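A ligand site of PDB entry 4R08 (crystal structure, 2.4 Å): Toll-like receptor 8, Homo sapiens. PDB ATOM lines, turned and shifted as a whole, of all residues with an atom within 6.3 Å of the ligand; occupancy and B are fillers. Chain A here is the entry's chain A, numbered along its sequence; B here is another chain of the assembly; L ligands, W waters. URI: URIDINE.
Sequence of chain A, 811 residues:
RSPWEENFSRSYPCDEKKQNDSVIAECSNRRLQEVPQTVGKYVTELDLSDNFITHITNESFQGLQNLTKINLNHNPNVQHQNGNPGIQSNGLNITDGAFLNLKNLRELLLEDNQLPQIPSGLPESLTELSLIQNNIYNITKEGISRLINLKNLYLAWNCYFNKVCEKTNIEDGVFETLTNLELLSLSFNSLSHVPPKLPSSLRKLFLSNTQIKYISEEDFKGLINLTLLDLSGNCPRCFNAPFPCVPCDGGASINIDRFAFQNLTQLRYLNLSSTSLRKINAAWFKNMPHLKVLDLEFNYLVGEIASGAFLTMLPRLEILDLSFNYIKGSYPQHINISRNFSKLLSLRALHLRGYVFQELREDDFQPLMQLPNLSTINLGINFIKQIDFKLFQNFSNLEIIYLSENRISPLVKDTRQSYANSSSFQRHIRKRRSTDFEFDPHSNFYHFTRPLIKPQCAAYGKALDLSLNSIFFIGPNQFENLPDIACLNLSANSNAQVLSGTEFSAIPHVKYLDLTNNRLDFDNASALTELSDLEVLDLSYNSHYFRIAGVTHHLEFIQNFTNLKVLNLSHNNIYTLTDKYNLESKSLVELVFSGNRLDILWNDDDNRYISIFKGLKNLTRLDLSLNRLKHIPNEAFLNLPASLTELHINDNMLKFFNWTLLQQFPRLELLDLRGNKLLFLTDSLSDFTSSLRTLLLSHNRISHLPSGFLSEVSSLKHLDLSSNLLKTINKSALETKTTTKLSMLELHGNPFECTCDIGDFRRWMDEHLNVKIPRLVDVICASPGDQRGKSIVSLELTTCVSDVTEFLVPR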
ATOM      1  N   ALA A 496       4.073   6.637 -35.175  1.00  0.00           N
ATOM      2  CA  ALA A 496       3.579   5.771 -34.095  1.00  0.00           C
ATOM      3  C   ALA A 496       3.340   6.503 -32.767  1.00  0.00           C
ATOM      4  O   ALA A 496       3.088   5.872 -31.733  1.00  0.00           O
ATOM      5  CB  ALA A 496       4.568   4.606 -33.897  1.00  0.00           C
ATOM      6  N   VAL A 498       2.080   8.974 -29.610  1.00  0.00           N
ATOM      7  CA  VAL A 498       0.886   9.328 -28.838  1.00  0.00           C
ATOM      8  C   VAL A 498       0.706  10.831 -28.953  1.00  0.00           C
ATOM      9  O   VAL A 498       1.498  11.590 -28.383  1.00  0.00           O
ATOM     10  CB  VAL A 498       1.067   8.965 -27.329  1.00  0.00           C
ATOM     11  CG1 VAL A 498      -0.115   9.444 -26.498  1.00  0.00           C
ATOM     12  CG2 VAL A 498       1.245   7.482 -27.146  1.00  0.00           C
ATOM     13  N   ASP A 521      -0.733   5.894 -31.963  1.00  0.00           N
ATOM     14  CA  ASP A 521      -1.067   5.246 -30.698  1.00  0.00           C
ATOM     15  C   ASP A 521      -1.931   6.184 -29.846  1.00  0.00           C
ATOM     16  O   ASP A 521      -1.442   7.194 -29.313  1.00  0.00           O
ATOM     17  CB  ASP A 521       0.215   4.917 -29.964  1.00  0.00           C
ATOM     18  CG  ASP A 521      -0.021   4.312 -28.621  1.00  0.00           C
ATOM     19  OD1 ASP A 521      -1.086   3.677 -28.412  1.00  0.00           O
ATOM     20  OD2 ASP A 521       0.898   4.399 -27.786  1.00  0.00           O
ATOM     21  N   ASP A 523      -3.341   7.043 -26.932  1.00  0.00           N
ATOM     22  CA  ASP A 523      -3.348   6.892 -25.511  1.00  0.00           C
ATOM     23  C   ASP A 523      -3.464   8.222 -24.774  1.00  0.00           C
ATOM     24  O   ASP A 523      -2.870   8.373 -23.698  1.00  0.00           O
ATOM     25  CB  ASP A 523      -2.071   6.212 -25.080  1.00  0.00           C
ATOM     26  CG  ASP A 523      -2.041   5.938 -23.609  1.00  0.00           C
ATOM     27  OD1 ASP A 523      -3.001   5.311 -23.123  1.00  0.00           O
ATOM     28  OD2 ASP A 523      -1.098   6.387 -22.952  1.00  0.00           O
ATOM     29  N   GLY A 550      -4.586  -5.336 -26.021  1.00  0.00           N
ATOM     30  CA  GLY A 550      -4.032  -5.019 -24.718  1.00  0.00           C
ATOM     31  C   GLY A 550      -3.452  -3.642 -24.469  1.00  0.00           C
ATOM     32  O   GLY A 550      -2.911  -3.361 -23.372  1.00  0.00           O
ATOM     33  N   VAL A 551      -3.529  -2.774 -25.464  1.00  0.00           N
ATOM     34  CA  VAL A 551      -2.956  -1.433 -25.331  1.00  0.00           C
ATOM     35  C   VAL A 551      -4.162  -0.508 -25.382  1.00  0.00           C
ATOM     36  O   VAL A 551      -5.179  -0.870 -25.907  1.00  0.00           O
ATOM     37  CB  VAL A 551      -1.959  -1.109 -26.487  1.00  0.00           C
ATOM     38  CG1 VAL A 551      -0.720  -1.977 -26.428  1.00  0.00           C
ATOM     39  CG2 VAL A 551      -2.611  -1.268 -27.864  1.00  0.00           C
ATOM     40  N   THR A 552      -4.062   0.675 -24.785  1.00  0.00           N
ATOM     41  CA  THR A 552      -5.209   1.592 -24.778  1.00  0.00           C
ATOM     42  C   THR A 552      -5.560   2.073 -26.175  1.00  0.00           C
ATOM     43  O   THR A 552      -4.698   2.193 -27.033  1.00  0.00           O
ATOM     44  CB  THR A 552      -4.909   2.811 -23.914  1.00  0.00           C
ATOM     45  OG1 THR A 552      -3.729   3.445 -24.405  1.00  0.00           O
ATOM     46  CG2 THR A 552      -4.666   2.385 -22.490  1.00  0.00           C
ATOM     47  N   PHE B 239      -9.533  -3.123 -16.602  1.00  0.00           N
ATOM     48  CA  PHE B 239      -9.194  -1.903 -17.298  1.00  0.00           C
ATOM     49  C   PHE B 239      -8.846  -2.231 -18.736  1.00  0.00           C
ATOM     50  O   PHE B 239      -7.959  -3.034 -19.003  1.00  0.00           O
ATOM     51  CB  PHE B 239      -8.030  -1.153 -16.648  1.00  0.00           C
ATOM     52  CG  PHE B 239      -7.514  -0.038 -17.499  1.00  0.00           C
ATOM     53  CD1 PHE B 239      -8.285   1.106 -17.697  1.00  0.00           C
ATOM     54  CD2 PHE B 239      -6.338  -0.186 -18.215  1.00  0.00           C
ATOM     55  CE1 PHE B 239      -7.847   2.114 -18.534  1.00  0.00           C
ATOM     56  CE2 PHE B 239      -5.892   0.830 -19.044  1.00  0.00           C
ATOM     57  CZ  PHE B 239      -6.639   1.986 -19.205  1.00  0.00           C
ATOM     58  N   ASN B 240      -9.554  -1.591 -19.662  1.00  0.00           N
ATOM     59  CA  ASN B 240      -9.301  -1.784 -21.068  1.00  0.00           C
ATOM     60  C   ASN B 240      -9.595  -3.210 -21.487  1.00  0.00           C
ATOM     61  O   ASN B 240      -8.932  -3.753 -22.377  1.00  0.00           O
ATOM     62  CB  ASN B 240      -7.842  -1.429 -21.372  1.00  0.00           C
ATOM     63  CG  ASN B 240      -7.513  -1.507 -22.833  1.00  0.00           C
ATOM     64  OD1 ASN B 240      -8.184  -0.905 -23.674  1.00  0.00           O
ATOM     65  ND2 ASN B 240      -6.476  -2.266 -23.158  1.00  0.00           N
ATOM     66  N   TYR B 326       1.164  -4.002 -16.137  1.00  0.00           N
ATOM     67  CA  TYR B 326       1.487  -2.589 -16.134  1.00  0.00           C
ATOM     68  C   TYR B 326       0.545  -1.779 -15.224  1.00  0.00           C
ATOM     69  O   TYR B 326      -0.630  -2.120 -15.092  1.00  0.00           O
ATOM     70  CB  TYR B 326       1.444  -2.040 -17.562  1.00  0.00           C
ATOM     71  CG  TYR B 326       0.060  -1.934 -18.179  1.00  0.00           C
ATOM     72  CD1 TYR B 326      -0.392  -2.865 -19.095  1.00  0.00           C
ATOM     73  CD2 TYR B 326      -0.765  -0.859 -17.904  1.00  0.00           C
ATOM     74  CE1 TYR B 326      -1.619  -2.729 -19.727  1.00  0.00           C
ATOM     75  CE2 TYR B 326      -2.005  -0.743 -18.490  1.00  0.00           C
ATOM     76  CZ  TYR B 326      -2.421  -1.657 -19.422  1.00  0.00           C
ATOM     77  OH  TYR B 326      -3.668  -1.556 -19.975  1.00  0.00           O
ATOM     78  N   ILE B 327       1.098  -0.765 -14.563  1.00  0.00           N
ATOM     79  CA  ILE B 327       0.288   0.241 -13.870  1.00  0.00           C
ATOM     80  C   ILE B 327      -0.161   1.274 -14.882  1.00  0.00           C
ATOM     81  O   ILE B 327       0.688   1.933 -15.509  1.00  0.00           O
ATOM     82  CB  ILE B 327       1.111   0.995 -12.803  1.00  0.00           C
ATOM     83  CG1 ILE B 327       1.463   0.088 -11.614  1.00  0.00           C
ATOM     84  CG2 ILE B 327       0.358   2.239 -12.328  1.00  0.00           C
ATOM     85  CD1 ILE B 327       2.909   0.172 -11.198  1.00  0.00           C
ATOM     86  N   LYS B 328      -1.464   1.488 -14.993  1.00  0.00           N
ATOM     87  CA  LYS B 328      -1.950   2.334 -16.051  1.00  0.00           C
ATOM     88  C   LYS B 328      -1.467   3.754 -15.835  1.00  0.00           C
ATOM     89  O   LYS B 328      -1.428   4.227 -14.691  1.00  0.00           O
ATOM     90  CB  LYS B 328      -3.472   2.271 -16.182  1.00  0.00           C
ATOM     91  CG  LYS B 328      -4.218   3.317 -15.407  1.00  0.00           C
ATOM     92  CD  LYS B 328      -5.694   3.256 -15.744  1.00  0.00           C
ATOM     93  CE  LYS B 328      -6.515   3.971 -14.713  1.00  0.00           C
ATOM     94  NZ  LYS B 328      -7.946   3.603 -14.825  1.00  0.00           N
ATOM     95  N   GLY B 329      -1.061   4.393 -16.930  1.00  0.00           N
ATOM     96  CA  GLY B 329      -0.514   5.741 -16.889  1.00  0.00           C
ATOM     97  C   GLY B 329       0.983   5.711 -16.689  1.00  0.00           C
ATOM     98  O   GLY B 329       1.716   6.392 -17.395  1.00  0.00           O
ATOM     99  N   SER B 330       1.445   4.895 -15.747  1.00  0.00           N
ATOM    100  CA  SER B 330       2.866   4.799 -15.420  1.00  0.00           C
ATOM    101  C   SER B 330       3.694   4.272 -16.597  1.00  0.00           C
ATOM    102  O   SER B 330       3.315   3.315 -17.278  1.00  0.00           O
ATOM    103  CB  SER B 330       3.043   3.889 -14.189  1.00  0.00           C
ATOM    104  OG  SER B 330       4.410   3.722 -13.835  1.00  0.00           O
ATOM    105  N   TYR B 331       4.822   4.919 -16.842  1.00  0.00           N
ATOM    106  CA  TYR B 331       5.689   4.582 -17.953  1.00  0.00           C
ATOM    107  C   TYR B 331       7.100   4.809 -17.438  1.00  0.00           C
ATOM    108  O   TYR B 331       7.767   5.766 -17.843  1.00  0.00           O
ATOM    109  CB  TYR B 331       5.360   5.465 -19.190  1.00  0.00           C
ATOM    110  CG  TYR B 331       6.135   5.146 -20.472  1.00  0.00           C
ATOM    111  CD1 TYR B 331       6.398   3.842 -20.856  1.00  0.00           C
ATOM    112  CD2 TYR B 331       6.522   6.159 -21.338  1.00  0.00           C
ATOM    113  CE1 TYR B 331       7.096   3.564 -22.019  1.00  0.00           C
ATOM    114  CE2 TYR B 331       7.206   5.894 -22.513  1.00  0.00           C
ATOM    115  CZ  TYR B 331       7.478   4.589 -22.856  1.00  0.00           C
ATOM    116  OH  TYR B 331       8.155   4.316 -24.039  1.00  0.00           O
ATOM    117  N   VAL B 356       5.555  -2.310 -19.656  1.00  0.00           N
ATOM    118  CA  VAL B 356       5.501  -0.947 -20.181  1.00  0.00           C
ATOM    119  C   VAL B 356       6.542  -0.016 -19.566  1.00  0.00           C
ATOM    120  O   VAL B 356       6.382   0.466 -18.441  1.00  0.00           O
ATOM    121  CB  VAL B 356       4.101  -0.362 -20.068  1.00  0.00           C
ATOM    122  CG1 VAL B 356       4.087   1.064 -20.587  1.00  0.00           C
ATOM    123  CG2 VAL B 356       3.120  -1.234 -20.851  1.00  0.00           C
ATOM    124  N   ASN B 382       5.985  -3.592 -24.918  1.00  0.00           N
ATOM    125  CA  ASN B 382       6.348  -2.776 -23.753  1.00  0.00           C
ATOM    126  C   ASN B 382       6.561  -1.297 -24.060  1.00  0.00           C
ATOM    127  O   ASN B 382       6.942  -0.540 -23.170  1.00  0.00           O
ATOM    128  CB  ASN B 382       7.608  -3.326 -23.131  1.00  0.00           C
ATOM    129  CG  ASN B 382       7.347  -4.539 -22.288  1.00  0.00           C
ATOM    130  OD1 ASN B 382       6.798  -4.420 -21.197  1.00  0.00           O
ATOM    131  ND2 ASN B 382       7.722  -5.703 -22.774  1.00  0.00           N
ATOM    132  N   PHE B 383       6.368  -0.887 -25.312  1.00  0.00           N
ATOM    133  CA  PHE B 383       6.666   0.467 -25.725  1.00  0.00           C
ATOM    134  C   PHE B 383       8.091   0.900 -25.379  1.00  0.00           C
ATOM    135  O   PHE B 383       8.319   2.068 -25.052  1.00  0.00           O
ATOM    136  CB  PHE B 383       5.688   1.448 -25.108  1.00  0.00           C
ATOM    137  CG  PHE B 383       4.263   1.247 -25.525  1.00  0.00           C
ATOM    138  CD1 PHE B 383       3.814   1.743 -26.756  1.00  0.00           C
ATOM    139  CD2 PHE B 383       3.356   0.630 -24.688  1.00  0.00           C
ATOM    140  CE1 PHE B 383       2.499   1.576 -27.145  1.00  0.00           C
ATOM    141  CE2 PHE B 383       2.030   0.497 -25.052  1.00  0.00           C
ATOM    142  CZ  PHE B 383       1.612   0.936 -26.306  1.00  0.00           C
ATOM    143  N   ARG B 407       9.214   0.432 -29.251  1.00  0.00           N
ATOM    144  CA  ARG B 407       9.520   1.728 -29.857  1.00  0.00           C
ATOM    145  C   ARG B 407      11.007   1.856 -30.133  1.00  0.00           C
ATOM    146  O   ARG B 407      11.601   2.932 -30.025  1.00  0.00           O
ATOM    147  CB  ARG B 407       9.063   2.868 -28.975  1.00  0.00           C
ATOM    148  CG  ARG B 407       7.553   2.997 -28.835  1.00  0.00           C
ATOM    149  CD  ARG B 407       7.198   4.332 -28.197  1.00  0.00           C
ATOM    150  NE  ARG B 407       5.754   4.610 -28.088  1.00  0.00           N
ATOM    151  CZ  ARG B 407       4.987   4.971 -29.103  1.00  0.00           C
ATOM    152  NH1 ARG B 407       5.499   5.004 -30.320  1.00  0.00           N
ATOM    153  NH2 ARG B 407       3.698   5.288 -28.918  1.00  0.00           N
HETATM  154  N1  URI L   1       1.657   3.521 -22.893  1.00  0.00           N
HETATM  155  C2  URI L   1       1.095   3.585 -24.203  1.00  0.00           C
HETATM  156  N3  URI L   1       1.831   4.099 -25.194  1.00  0.00           N
HETATM  157  C4  URI L   1       3.073   4.567 -24.997  1.00  0.00           C
HETATM  158  C5  URI L   1       3.653   4.486 -23.735  1.00  0.00           C
HETATM  159  C6  URI L   1       2.925   3.944 -22.699  1.00  0.00           C
HETATM  160  O2  URI L   1      -0.063   3.143 -24.461  1.00  0.00           O
HETATM  161  O4  URI L   1       3.725   5.066 -25.940  1.00  0.00           O
HETATM  162  C1' URI L   1       0.967   2.945 -21.751  1.00  0.00           C
HETATM  163  C2' URI L   1      -0.388   3.584 -21.528  1.00  0.00           C
HETATM  164  C3' URI L   1      -1.261   2.471 -21.022  1.00  0.00           C
HETATM  165  C4' URI L   1      -0.521   1.187 -21.408  1.00  0.00           C
HETATM  166  O2' URI L   1      -0.261   4.585 -20.534  1.00  0.00           O
HETATM  167  O3' URI L   1      -1.364   2.654 -19.583  1.00  0.00           O
HETATM  168  O4' URI L   1       0.736   1.571 -21.980  1.00  0.00           O
HETATM  169  C5' URI L   1      -1.246   0.238 -22.365  1.00  0.00           C
HETATM  170  O5' URI L   1      -1.281   0.738 -23.703  1.00  0.00           O
HETATM  171  O   HOH W   1      -1.966   2.600 -26.172  1.00  0.00           O
HETATM  172  O   HOH W   2       0.841   2.109 -18.521  1.00  0.00           O
HETATM  173  O   HOH W   3       5.088   7.484 -26.026  1.00  0.00           O
HETATM  174  O   HOH W   4      -2.809   4.669 -19.621  1.00  0.00           O
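Merely in contact with the ligand: Val 498 (3.7 Å), Val 551 (3.2 Å), Tyr 326 of chain B (3.6 Å), Lys 328 of chain B (3.6 Å), Tyr 331 of chain B (3.9 Å), Val 356 of chain B (3.7 Å) and Phe 383 of chain B (3.3 Å).
Hydrophobic or aromatic side chains within 4 Å of the ligand: Val 498, Val 551, Tyr 326 of chain B, Tyr 331 of chain B, Val 356 of chain B and Phe 383 of chain B.
Along chain A the residues within 4 Å of the ligand span positions 498 to 552.
The nearest printed residue that does not touch the ligand is Gly 550 (4.1 Å).
Water W4 bridges an oxygen (O3') of the ligand (2.5 Å) and the backbone NH of Gly 329 of chain B (3.2 Å).
Water W2 lies within hydrogen-bond range of an oxygen (O3') of the ligand (2.5 Å), the backbone carbonyl oxygen (O) of Ser 330 of chain B (3.0 Å) and the backbone NH (N) of Gly 329 of chain B (3.4 Å).
Water W1 lies within hydrogen-bond range of an oxygen (O2) of the ligand (2.6 Å), the side-chain hydroxyl (OG1) of Thr 552 (2.6 Å) and the side-chain carboxylate (OD1) of Asp 521 (2.6 Å).
The side-chain carboxylate (OD2) of Asp 521 lies within hydrogen-bond range of a nitrogen (N3) of the ligand, 2.8 Å away.
An oxygen (O5') of the ligand is in hydrogen-bond range of the backbone NH (N) of Thr 552 (3.0 Å).
NH2 of Arg 407 of chain B lies within hydrogen-bond range of O4 of the ligand (3.0 Å).
O2' of the ligand is in hydrogen-bond range of OD2 of Asp 523 (3.1 Å).
The backbone NH (N) of Gly 329 of chain B sits at hydrogen-bond distance from an oxygen (O3') of the ligand (3.2 Å).
The guanidinium group of Arg 407 of chain B lies within salt-bridge range of the side-chain carboxylate of Asp 521 (3.1 Å).
The backbone carbonyl oxygen (O) of Ala 496 is in hydrogen-bond range of the guanidinium group (NH1) of Arg 407 of chain B, 2.9 Å away.
ND2 of Asn 240 of chain B sits at hydrogen-bond distance from O of Val 551.
The backbone carbonyl oxygen of Phe 383 of chain B sits at hydrogen-bond distance from the side-chain hydroxyl of Tyr 331 of chain B (2.5 Å).
OD1 of Asn 382 of chain B sits at hydrogen-bond distance from N of Val 356 of chain B, 2.9 Å away.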
